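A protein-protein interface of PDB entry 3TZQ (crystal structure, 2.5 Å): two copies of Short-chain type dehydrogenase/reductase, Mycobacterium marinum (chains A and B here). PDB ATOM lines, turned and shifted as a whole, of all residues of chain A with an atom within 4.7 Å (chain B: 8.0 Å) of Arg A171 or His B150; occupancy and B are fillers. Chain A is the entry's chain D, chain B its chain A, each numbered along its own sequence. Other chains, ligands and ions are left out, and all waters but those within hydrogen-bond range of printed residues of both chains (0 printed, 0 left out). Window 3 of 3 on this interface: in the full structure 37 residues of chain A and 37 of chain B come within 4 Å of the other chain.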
ATOM      1  N   GLU A 167      24.377 -13.047   0.004  1.00  0.00           N
ATOM      2  CA  GLU A 167      24.272 -12.789   1.455  1.00  0.00           C
ATOM      3  C   GLU A 167      22.817 -12.566   1.889  1.00  0.00           C
ATOM      4  O   GLU A 167      22.375 -13.131   2.892  1.00  0.00           O
ATOM      5  CB  GLU A 167      25.189 -11.623   1.885  1.00  0.00           C
ATOM      6  CG  GLU A 167      26.673 -12.018   1.843  1.00  0.00           C
ATOM      7  CD  GLU A 167      27.661 -10.960   2.323  1.00  0.00           C
ATOM      8  OE1 GLU A 167      27.268  -9.925   2.901  1.00  0.00           O
ATOM      9  OE2 GLU A 167      28.876 -11.186   2.133  1.00  0.00           O
ATOM     10  N   THR A 168      22.071 -11.779   1.115  1.00  0.00           N
ATOM     11  CA  THR A 168      20.649 -11.584   1.383  1.00  0.00           C
ATOM     12  C   THR A 168      19.847 -12.852   1.133  1.00  0.00           C
ATOM     13  O   THR A 168      18.969 -13.230   1.947  1.00  0.00           O
ATOM     14  CB  THR A 168      20.078 -10.436   0.542  1.00  0.00           C
ATOM     15  OG1 THR A 168      20.739  -9.229   0.932  1.00  0.00           O
ATOM     16  CG2 THR A 168      18.563 -10.277   0.763  1.00  0.00           C
ATOM     17  N   LEU A 169      20.171 -13.508   0.020  1.00  0.00           N
ATOM     18  CA  LEU A 169      19.595 -14.807  -0.268  1.00  0.00           C
ATOM     19  C   LEU A 169      19.744 -15.726   0.933  1.00  0.00           C
ATOM     20  O   LEU A 169      18.806 -16.434   1.283  1.00  0.00           O
ATOM     21  CB  LEU A 169      20.228 -15.448  -1.506  1.00  0.00           C
ATOM     22  CG  LEU A 169      19.571 -16.746  -1.998  1.00  0.00           C
ATOM     23  CD1 LEU A 169      18.062 -16.594  -2.125  1.00  0.00           C
ATOM     24  CD2 LEU A 169      20.189 -17.168  -3.314  1.00  0.00           C
ATOM     25  N   THR A 170      20.920 -15.696   1.568  1.00  0.00           N
ATOM     26  CA  THR A 170      21.192 -16.606   2.661  1.00  0.00           C
ATOM     27  C   THR A 170      20.229 -16.338   3.813  1.00  0.00           C
ATOM     28  O   THR A 170      19.662 -17.268   4.395  1.00  0.00           O
ATOM     29  CB  THR A 170      22.656 -16.520   3.139  1.00  0.00           C
ATOM     30  OG1 THR A 170      23.528 -17.059   2.119  1.00  0.00           O
ATOM     31  CG2 THR A 170      22.837 -17.282   4.460  1.00  0.00           C
ATOM     32  N   ARG A 171      20.023 -15.065   4.115  1.00  0.00           N
ATOM     33  CA  ARG A 171      19.042 -14.695   5.122  1.00  0.00           C
ATOM     34  C   ARG A 171      17.626 -15.177   4.746  1.00  0.00           C
ATOM     35  O   ARG A 171      16.902 -15.717   5.588  1.00  0.00           O
ATOM     36  CB  ARG A 171      19.087 -13.176   5.389  1.00  0.00           C
ATOM     37  CG  ARG A 171      20.251 -12.760   6.283  1.00  0.00           C
ATOM     38  CD  ARG A 171      20.217 -11.285   6.661  1.00  0.00           C
ATOM     39  NE  ARG A 171      20.693 -10.461   5.556  1.00  0.00           N
ATOM     40  CZ  ARG A 171      21.939  -9.989   5.383  1.00  0.00           C
ATOM     41  NH1 ARG A 171      22.920 -10.219   6.262  1.00  0.00           N
ATOM     42  NH2 ARG A 171      22.206  -9.259   4.298  1.00  0.00           N
ATOM     43  N   TYR A 172      17.252 -15.014   3.474  1.00  0.00           N
ATOM     44  CA  TYR A 172      15.921 -15.419   3.020  1.00  0.00           C
ATOM     45  C   TYR A 172      15.717 -16.922   3.105  1.00  0.00           C
ATOM     46  O   TYR A 172      14.650 -17.402   3.546  1.00  0.00           O
ATOM     47  CB  TYR A 172      15.624 -14.863   1.620  1.00  0.00           C
ATOM     48  CG  TYR A 172      15.083 -13.457   1.695  1.00  0.00           C
ATOM     49  CD1 TYR A 172      15.897 -12.413   2.071  1.00  0.00           C
ATOM     50  CD2 TYR A 172      13.754 -13.192   1.469  1.00  0.00           C
ATOM     51  CE1 TYR A 172      15.407 -11.128   2.186  1.00  0.00           C
ATOM     52  CE2 TYR A 172      13.260 -11.922   1.585  1.00  0.00           C
ATOM     53  CZ  TYR A 172      14.092 -10.889   1.940  1.00  0.00           C
ATOM     54  OH  TYR A 172      13.604  -9.618   2.065  1.00  0.00           O
ATOM     55  N   VAL A 173      16.746 -17.669   2.737  1.00  0.00           N
ATOM     56  CA  VAL A 173      16.687 -19.121   2.890  1.00  0.00           C
ATOM     57  C   VAL A 173      16.532 -19.531   4.373  1.00  0.00           C
ATOM     58  O   VAL A 173      15.672 -20.352   4.710  1.00  0.00           O
ATOM     59  CB  VAL A 173      17.917 -19.785   2.255  1.00  0.00           C
ATOM     60  CG1 VAL A 173      17.961 -21.271   2.598  1.00  0.00           C
ATOM     61  CG2 VAL A 173      17.924 -19.522   0.740  1.00  0.00           C
ATOM     62  N   ALA A 174      17.327 -18.931   5.259  1.00  0.00           N
ATOM     63  CA  ALA A 174      17.227 -19.195   6.710  1.00  0.00           C
ATOM     64  C   ALA A 174      15.851 -18.868   7.313  1.00  0.00           C
ATOM     65  O   ALA A 174      15.323 -19.625   8.135  1.00  0.00           O
ATOM     66  CB  ALA A 174      18.301 -18.441   7.464  1.00  0.00           C
ATOM     67  N   THR A 175      15.294 -17.723   6.935  1.00  0.00           N
ATOM     68  CA  THR A 175      14.052 -17.241   7.532  1.00  0.00           C
ATOM     69  C   THR A 175      12.920 -18.115   7.044  1.00  0.00           C
ATOM     70  O   THR A 175      12.006 -18.458   7.801  1.00  0.00           O
ATOM     71  CB  THR A 175      13.766 -15.791   7.108  1.00  0.00           C
ATOM     72  OG1 THR A 175      14.836 -14.940   7.522  1.00  0.00           O
ATOM     73  CG2 THR A 175      12.479 -15.271   7.709  1.00  0.00           C
ATOM     74  N   GLY A 241      21.587 -17.988   9.278  1.00  0.00           N
ATOM     75  CA  GLY A 241      21.256 -16.708   8.651  1.00  0.00           C
ATOM     76  C   GLY A 241      22.300 -15.624   8.842  1.00  0.00           C
ATOM     77  O   GLY A 241      21.976 -14.442   8.728  1.00  0.00           O
ATOM     78  N   VAL A 243      26.373 -13.940   8.253  1.00  0.00           N
ATOM     79  CA  VAL A 243      27.446 -13.819   7.280  1.00  0.00           C
ATOM     80  C   VAL A 243      28.713 -13.733   8.089  1.00  0.00           C
ATOM     81  O   VAL A 243      28.907 -12.763   8.819  1.00  0.00           O
ATOM     82  CB  VAL A 243      27.306 -12.588   6.358  1.00  0.00           C
ATOM     83  CG1 VAL A 243      28.452 -12.591   5.346  1.00  0.00           C
ATOM     84  CG2 VAL A 243      25.953 -12.593   5.653  1.00  0.00           C
ATOM     85  N   VAL B 103      11.837 -18.892  -2.060  1.00  0.00           N
ATOM     86  CA  VAL B 103      12.982 -19.337  -2.850  1.00  0.00           C
ATOM     87  C   VAL B 103      12.636 -20.578  -3.651  1.00  0.00           C
ATOM     88  O   VAL B 103      12.866 -20.619  -4.862  1.00  0.00           O
ATOM     89  CB  VAL B 103      14.236 -19.598  -1.994  1.00  0.00           C
ATOM     90  CG1 VAL B 103      15.293 -20.333  -2.804  1.00  0.00           C
ATOM     91  CG2 VAL B 103      14.790 -18.291  -1.465  1.00  0.00           C
ATOM     92  N   SER B 145      17.729   1.491  -1.788  1.00  0.00           N
ATOM     93  CA  SER B 145      17.796   0.070  -1.399  1.00  0.00           C
ATOM     94  C   SER B 145      16.493  -0.210  -0.684  1.00  0.00           C
ATOM     95  O   SER B 145      15.467   0.293  -1.105  1.00  0.00           O
ATOM     96  CB  SER B 145      18.987  -0.172  -0.476  1.00  0.00           C
ATOM     97  OG  SER B 145      19.124  -1.538  -0.137  1.00  0.00           O
ATOM     98  N   SER B 146      16.520  -0.975   0.397  1.00  0.00           N
ATOM     99  CA  SER B 146      15.319  -1.284   1.156  1.00  0.00           C
ATOM    100  C   SER B 146      15.709  -2.080   2.378  1.00  0.00           C
ATOM    101  O   SER B 146      16.650  -2.849   2.323  1.00  0.00           O
ATOM    102  CB  SER B 146      14.386  -2.144   0.330  1.00  0.00           C
ATOM    103  OG  SER B 146      13.624  -2.999   1.141  1.00  0.00           O
ATOM    104  N   ALA B 147      14.959  -1.944   3.463  1.00  0.00           N
ATOM    105  CA  ALA B 147      15.233  -2.712   4.653  1.00  0.00           C
ATOM    106  C   ALA B 147      15.174  -4.215   4.373  1.00  0.00           C
ATOM    107  O   ALA B 147      15.723  -5.001   5.147  1.00  0.00           O
ATOM    108  CB  ALA B 147      14.253  -2.342   5.760  1.00  0.00           C
ATOM    109  N   THR B 148      14.508  -4.613   3.285  1.00  0.00           N
ATOM    110  CA  THR B 148      14.304  -6.024   3.002  1.00  0.00           C
ATOM    111  C   THR B 148      15.593  -6.761   2.653  1.00  0.00           C
ATOM    112  O   THR B 148      15.648  -7.977   2.789  1.00  0.00           O
ATOM    113  CB  THR B 148      13.247  -6.258   1.901  1.00  0.00           C
ATOM    114  OG1 THR B 148      13.565  -5.480   0.746  1.00  0.00           O
ATOM    115  CG2 THR B 148      11.876  -5.892   2.412  1.00  0.00           C
ATOM    116  N   ALA B 149      16.613  -6.020   2.224  1.00  0.00           N
ATOM    117  CA  ALA B 149      17.947  -6.584   1.978  1.00  0.00           C
ATOM    118  C   ALA B 149      18.585  -7.068   3.269  1.00  0.00           C
ATOM    119  O   ALA B 149      19.448  -7.918   3.240  1.00  0.00           O
ATOM    120  CB  ALA B 149      18.868  -5.576   1.303  1.00  0.00           C
ATOM    121  N   HIS B 150      18.155  -6.526   4.397  1.00  0.00           N
ATOM    122  CA  HIS B 150      18.838  -6.782   5.668  1.00  0.00           C
ATOM    123  C   HIS B 150      18.138  -7.743   6.565  1.00  0.00           C
ATOM    124  O   HIS B 150      18.755  -8.244   7.491  1.00  0.00           O
ATOM    125  CB  HIS B 150      19.067  -5.478   6.431  1.00  0.00           C
ATOM    126  CG  HIS B 150      20.115  -4.606   5.810  1.00  0.00           C
ATOM    127  ND1 HIS B 150      21.447  -4.842   5.971  1.00  0.00           N
ATOM    128  CD2 HIS B 150      20.002  -3.491   4.960  1.00  0.00           C
ATOM    129  CE1 HIS B 150      22.147  -3.915   5.275  1.00  0.00           C
ATOM    130  NE2 HIS B 150      21.257  -3.087   4.658  1.00  0.00           N
ATOM    131  N   ALA B 151      16.854  -7.981   6.324  1.00  0.00           N
ATOM    132  CA  ALA B 151      16.059  -8.795   7.214  1.00  0.00           C
ATOM    133  C   ALA B 151      14.940  -9.389   6.391  1.00  0.00           C
ATOM    134  O   ALA B 151      14.249  -8.662   5.702  1.00  0.00           O
ATOM    135  CB  ALA B 151      15.515  -7.938   8.335  1.00  0.00           C
ATOM    136  N   ALA B 152      14.782 -10.705   6.448  1.00  0.00           N
ATOM    137  CA  ALA B 152      13.995 -11.460   5.459  1.00  0.00           C
ATOM    138  C   ALA B 152      12.601 -11.785   5.900  1.00  0.00           C
ATOM    139  O   ALA B 152      12.267 -11.718   7.079  1.00  0.00           O
ATOM    140  CB  ALA B 152      14.692 -12.759   5.129  1.00  0.00           C
ATOM    141  N   TYR B 153      11.793 -12.158   4.921  1.00  0.00           N
ATOM    142  CA  TYR B 153      10.481 -12.712   5.170  1.00  0.00           C
ATOM    143  C   TYR B 153       9.988 -13.543   3.975  1.00  0.00           C
ATOM    144  O   TYR B 153      10.765 -13.928   3.108  1.00  0.00           O
ATOM    145  CB  TYR B 153       9.492 -11.623   5.596  1.00  0.00           C
ATOM    146  CG  TYR B 153       9.059 -10.653   4.530  1.00  0.00           C
ATOM    147  CD1 TYR B 153       7.721 -10.334   4.358  1.00  0.00           C
ATOM    148  CD2 TYR B 153       9.986 -10.029   3.735  1.00  0.00           C
ATOM    149  CE1 TYR B 153       7.322  -9.435   3.396  1.00  0.00           C
ATOM    150  CE2 TYR B 153       9.597  -9.129   2.764  1.00  0.00           C
ATOM    151  CZ  TYR B 153       8.270  -8.824   2.604  1.00  0.00           C
ATOM    152  OH  TYR B 153       7.936  -7.907   1.625  1.00  0.00           O
ATOM    153  N   THR B 157      12.021 -12.087  -2.276  1.00  0.00           N
ATOM    154  CA  THR B 157      13.390 -12.645  -2.281  1.00  0.00           C
ATOM    155  C   THR B 157      14.293 -12.036  -3.368  1.00  0.00           C
ATOM    156  O   THR B 157      15.419 -11.652  -3.080  1.00  0.00           O
ATOM    157  CB  THR B 157      13.352 -14.168  -2.544  1.00  0.00           C
ATOM    158  OG1 THR B 157      12.383 -14.779  -1.685  1.00  0.00           O
ATOM    159  CG2 THR B 157      14.706 -14.798  -2.348  1.00  0.00           C
ATOM    160  N   ALA B 160      14.566  -8.160  -2.759  1.00  0.00           N
ATOM    161  CA  ALA B 160      15.497  -7.983  -1.639  1.00  0.00           C
ATOM    162  C   ALA B 160      16.974  -8.124  -2.049  1.00  0.00           C
ATOM    163  O   ALA B 160      17.812  -7.288  -1.669  1.00  0.00           O
ATOM    164  CB  ALA B 160      15.171  -8.944  -0.506  1.00  0.00           C
ATOM    165  N   CYS B 161      17.274  -9.177  -2.824  1.00  0.00           N
ATOM    166  CA  CYS B 161      18.649  -9.512  -3.203  1.00  0.00           C
ATOM    167  C   CYS B 161      19.223  -8.456  -4.174  1.00  0.00           C
ATOM    168  O   CYS B 161      20.411  -8.138  -4.119  1.00  0.00           O
ATOM    169  CB  CYS B 161      18.709 -10.916  -3.806  1.00  0.00           C
ATOM    170  SG  CYS B 161      18.297 -12.271  -2.661  1.00  0.00           S
ATOM    171  N   LYS B 163      18.354  -5.289  -4.093  1.00  0.00           N
ATOM    172  CA  LYS B 163      18.669  -4.167  -3.247  1.00  0.00           C
ATOM    173  C   LYS B 163      20.026  -4.369  -2.593  1.00  0.00           C
ATOM    174  O   LYS B 163      20.799  -3.421  -2.498  1.00  0.00           O
ATOM    175  CB  LYS B 163      17.580  -3.904  -2.203  1.00  0.00           C
ATOM    176  CG  LYS B 163      16.267  -3.378  -2.785  1.00  0.00           C
ATOM    177  CD  LYS B 163      16.423  -2.487  -4.031  1.00  0.00           C
ATOM    178  CE  LYS B 163      15.142  -1.717  -4.354  1.00  0.00           C
ATOM    179  NZ  LYS B 163      15.382  -0.657  -5.373  1.00  0.00           N
ATOM    180  N   ALA B 164      20.339  -5.595  -2.193  1.00  0.00           N
ATOM    181  CA  ALA B 164      21.679  -5.894  -1.648  1.00  0.00           C
ATOM    182  C   ALA B 164      22.823  -5.606  -2.658  1.00  0.00           C
ATOM    183  O   ALA B 164      23.858  -5.044  -2.286  1.00  0.00           O
ATOM    184  CB  ALA B 164      21.745  -7.347  -1.176  1.00  0.00           C
ATOM    185  N   GLU B 167      23.370  -1.982  -2.851  1.00  0.00           N
ATOM    186  CA  GLU B 167      24.113  -1.479  -1.706  1.00  0.00           C
ATOM    187  C   GLU B 167      25.622  -1.602  -1.949  1.00  0.00           C
ATOM    188  O   GLU B 167      26.346  -0.626  -1.747  1.00  0.00           O
ATOM    189  CB  GLU B 167      23.667  -2.133  -0.380  1.00  0.00           C
ATOM    190  CG  GLU B 167      22.420  -1.482   0.231  1.00  0.00           C
ATOM    191  CD  GLU B 167      21.913  -2.151   1.520  1.00  0.00           C
ATOM    192  OE1 GLU B 167      22.606  -2.986   2.172  1.00  0.00           O
ATOM    193  OE2 GLU B 167      20.765  -1.840   1.902  1.00  0.00           O
ATOM    194  N   ARG B 171      28.972   1.349  -2.639  1.00  0.00           N
ATOM    195  CA  ARG B 171      30.342   1.370  -2.132  1.00  0.00           C
ATOM    196  C   ARG B 171      31.399   1.380  -3.255  1.00  0.00           C
ATOM    197  O   ARG B 171      32.400   2.078  -3.157  1.00  0.00           O
ATOM    198  CB  ARG B 171      30.556   0.213  -1.143  1.00  0.00           C
ATOM    199  CG  ARG B 171      29.875   0.486   0.197  1.00  0.00           C
ATOM    200  CD  ARG B 171      30.143  -0.558   1.276  1.00  0.00           C
ATOM    201  NE  ARG B 171      29.432  -1.787   0.992  1.00  0.00           N
ATOM    202  CZ  ARG B 171      28.277  -2.189   1.531  1.00  0.00           C
ATOM    203  NH1 ARG B 171      27.636  -1.487   2.456  1.00  0.00           N
ATOM    204  NH2 ARG B 171      27.759  -3.354   1.132  1.00  0.00           N
ATOM    205  N   ILE B 187      19.817   4.626   0.583  1.00  0.00           N
ATOM    206  CA  ILE B 187      18.796   4.694   1.602  1.00  0.00           C
ATOM    207  C   ILE B 187      18.040   3.357   1.603  1.00  0.00           C
ATOM    208  O   ILE B 187      17.575   2.889   0.535  1.00  0.00           O
ATOM    209  CB  ILE B 187      17.777   5.822   1.298  1.00  0.00           C
ATOM    210  CG1 ILE B 187      18.458   7.195   1.228  1.00  0.00           C
ATOM    211  CG2 ILE B 187      16.626   5.798   2.309  1.00  0.00           C
ATOM    212  CD1 ILE B 187      17.541   8.291   0.695  1.00  0.00           C
ATOM    213  N   ALA B 188      17.951   2.750   2.793  1.00  0.00           N
ATOM    214  CA  ALA B 188      17.078   1.579   3.036  1.00  0.00           C
ATOM    215  C   ALA B 188      15.812   2.015   3.777  1.00  0.00           C
ATOM    216  O   ALA B 188      15.810   2.072   4.989  1.00  0.00           O
ATOM    217  CB  ALA B 188      17.796   0.512   3.856  1.00  0.00           C
ATOM    218  N   VAL B 243      25.082   3.251   3.603  1.00  0.00           N
ATOM    219  CA  VAL B 243      23.705   2.784   3.518  1.00  0.00           C
ATOM    220  C   VAL B 243      23.011   3.262   4.799  1.00  0.00           C
ATOM    221  O   VAL B 243      23.385   2.869   5.916  1.00  0.00           O
ATOM    222  CB  VAL B 243      23.634   1.243   3.410  1.00  0.00           C
ATOM    223  CG1 VAL B 243      22.189   0.780   3.365  1.00  0.00           C
ATOM    224  CG2 VAL B 243      24.407   0.766   2.168  1.00  0.00           C
ATOM    225  N   ILE B 244      22.021   4.135   4.639  1.00  0.00           N
ATOM    226  CA  ILE B 244      21.401   4.799   5.765  1.00  0.00           C
ATOM    227  C   ILE B 244      19.946   4.384   5.835  1.00  0.00           C
ATOM    228  O   ILE B 244      19.192   4.559   4.883  1.00  0.00           O
ATOM    229  CB  ILE B 244      21.535   6.328   5.656  1.00  0.00           C
ATOM    230  CG1 ILE B 244      22.998   6.741   5.626  1.00  0.00           C
ATOM    231  CG2 ILE B 244      20.918   7.016   6.846  1.00  0.00           C
ATOM    232  CD1 ILE B 244      23.194   8.233   5.471  1.00  0.00           C
ATOM    233  N   ALA B 245      19.554   3.826   6.967  1.00  0.00           N
ATOM    234  CA  ALA B 245      18.200   3.358   7.136  1.00  0.00           C
ATOM    235  C   ALA B 245      17.289   4.523   7.491  1.00  0.00           C
ATOM    236  O   ALA B 245      17.553   5.244   8.440  1.00  0.00           O
ATOM    237  CB  ALA B 245      18.133   2.280   8.214  1.00  0.00           C
ATOM    238  N   ASP B 247      13.861   4.087   8.459  1.00  0.00           N
ATOM    239  CA  ASP B 247      12.926   3.008   8.774  1.00  0.00           C
ATOM    240  C   ASP B 247      12.382   3.044  10.201  1.00  0.00           C
ATOM    241  O   ASP B 247      11.919   2.016  10.732  1.00  0.00           O
ATOM    242  CB  ASP B 247      13.658   1.678   8.559  1.00  0.00           C
ATOM    243  CG  ASP B 247      14.835   1.467   9.556  1.00  0.00           C
ATOM    244  OD1 ASP B 247      15.115   2.308  10.447  1.00  0.00           O
ATOM    245  OD2 ASP B 247      15.502   0.419   9.435  1.00  0.00           O
ATOM    246  N   LEU B 251      14.788  -2.188  12.548  1.00  0.00           N
ATOM    247  CA  LEU B 251      15.750  -3.225  12.880  1.00  0.00           C
ATOM    248  C   LEU B 251      16.651  -2.851  14.079  1.00  0.00           C
ATOM    249  O   LEU B 251      17.617  -3.573  14.381  1.00  0.00           O
ATOM    250  CB  LEU B 251      16.566  -3.596  11.626  1.00  0.00           C
ATOM    251  CG  LEU B 251      15.775  -3.798  10.300  1.00  0.00           C
ATOM    252  CD1 LEU B 251      16.649  -4.299   9.146  1.00  0.00           C
ATOM    253  CD2 LEU B 251      14.603  -4.741  10.481  1.00  0.00           C
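The backbone carbonyl oxygen (O) of Ala B149 is in hydrogen-bond range of the guanidinium group (NH2) of Arg A171, 3.2 Å away. N of Leu A169 sits at hydrogen-bond distance from SG of Cys B161. The backbone carbonyl oxygen (O) of Ala B149 sits at hydrogen-bond distance from the side-chain hydroxyl (OG1) of Thr A168 (3.0 Å). O of Thr B148 lies within hydrogen-bond range of OH of Tyr A172 (2.7 Å).
OE1 of Glu B167 sits at hydrogen-bond distance from NE2 of His B150 (2.8 Å). The backbone carbonyl oxygen (O) of Arg A171 lies within hydrogen-bond range of the side-chain hydroxyl (OG1) of Thr A175 (2.9 Å). OG of Ser B146 is in hydrogen-bond range of OG1 of Thr B148 (2.5 Å). O of Thr B157 lies within hydrogen-bond range of SG of Cys B161, at 3.0 Å.
Among the printed residues, merely in contact across the chains: Thr A168 with Ala B160, Thr A168 with Cys B161, Thr A168 with Ala B164, Leu A169 with Val B103, Leu A169 with Thr B157, Arg A171 with His B150, Arg A171 with Ala B152, Tyr A172 with Ala B151, Tyr A172 with Ala B152, Tyr A172 with Tyr B153, Tyr A172 with Thr B157, Tyr A172 with Ala B160 and Thr A175 with Ala B152.
Of the printed residues of chain B, Thr A168 touches Ala B149 (3.0 Å), Ala B160 (3.9 Å), Cys B161 (3.97 Å) and Ala B164 (3.0 Å). Of chain B, only Ala B149 (3.2 Å), His B150 (3.5 Å) and Ala B152 (3.7 Å) come within 4 Å of Arg A171. Printed residues of chain A within 4 Å of Val B103: Leu A169. Printed residues of chain A within 4 Å of Ala B149: Thr A168 (3.0 Å) and Arg A171 (3.2 Å). Of the printed residues of chain A, Tyr B153 touches Tyr A172 (3.5 Å). Of the printed residues of chain A, Ala B164 touches Thr A168 (3.0 Å). Ile B187 touches none of the printed residues of chain A. The nearest residue of chain B that does not touch Arg A171 is Ala B151 (4.6 Å).
Printed residues of chain B that touch a printed residue of chain A: Val B103, Thr B148, Ala B149, His B150, Ala B151, Ala B152, Tyr B153, Thr B157, Ala B160, Cys B161 and Ala B164. Printed residues of chain A that touch a printed residue of chain B: Thr A168, Leu A169, Arg A171, Tyr A172 and Thr A175. Among the printed residues, 17 pairs touch across the chains. Among the printed residues, no Asp or Glu carboxylate lies within 4 Å of a Lys or Arg side-chain nitrogen of the other chain.
Positions printed for both chains: 167, 171 and 243.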
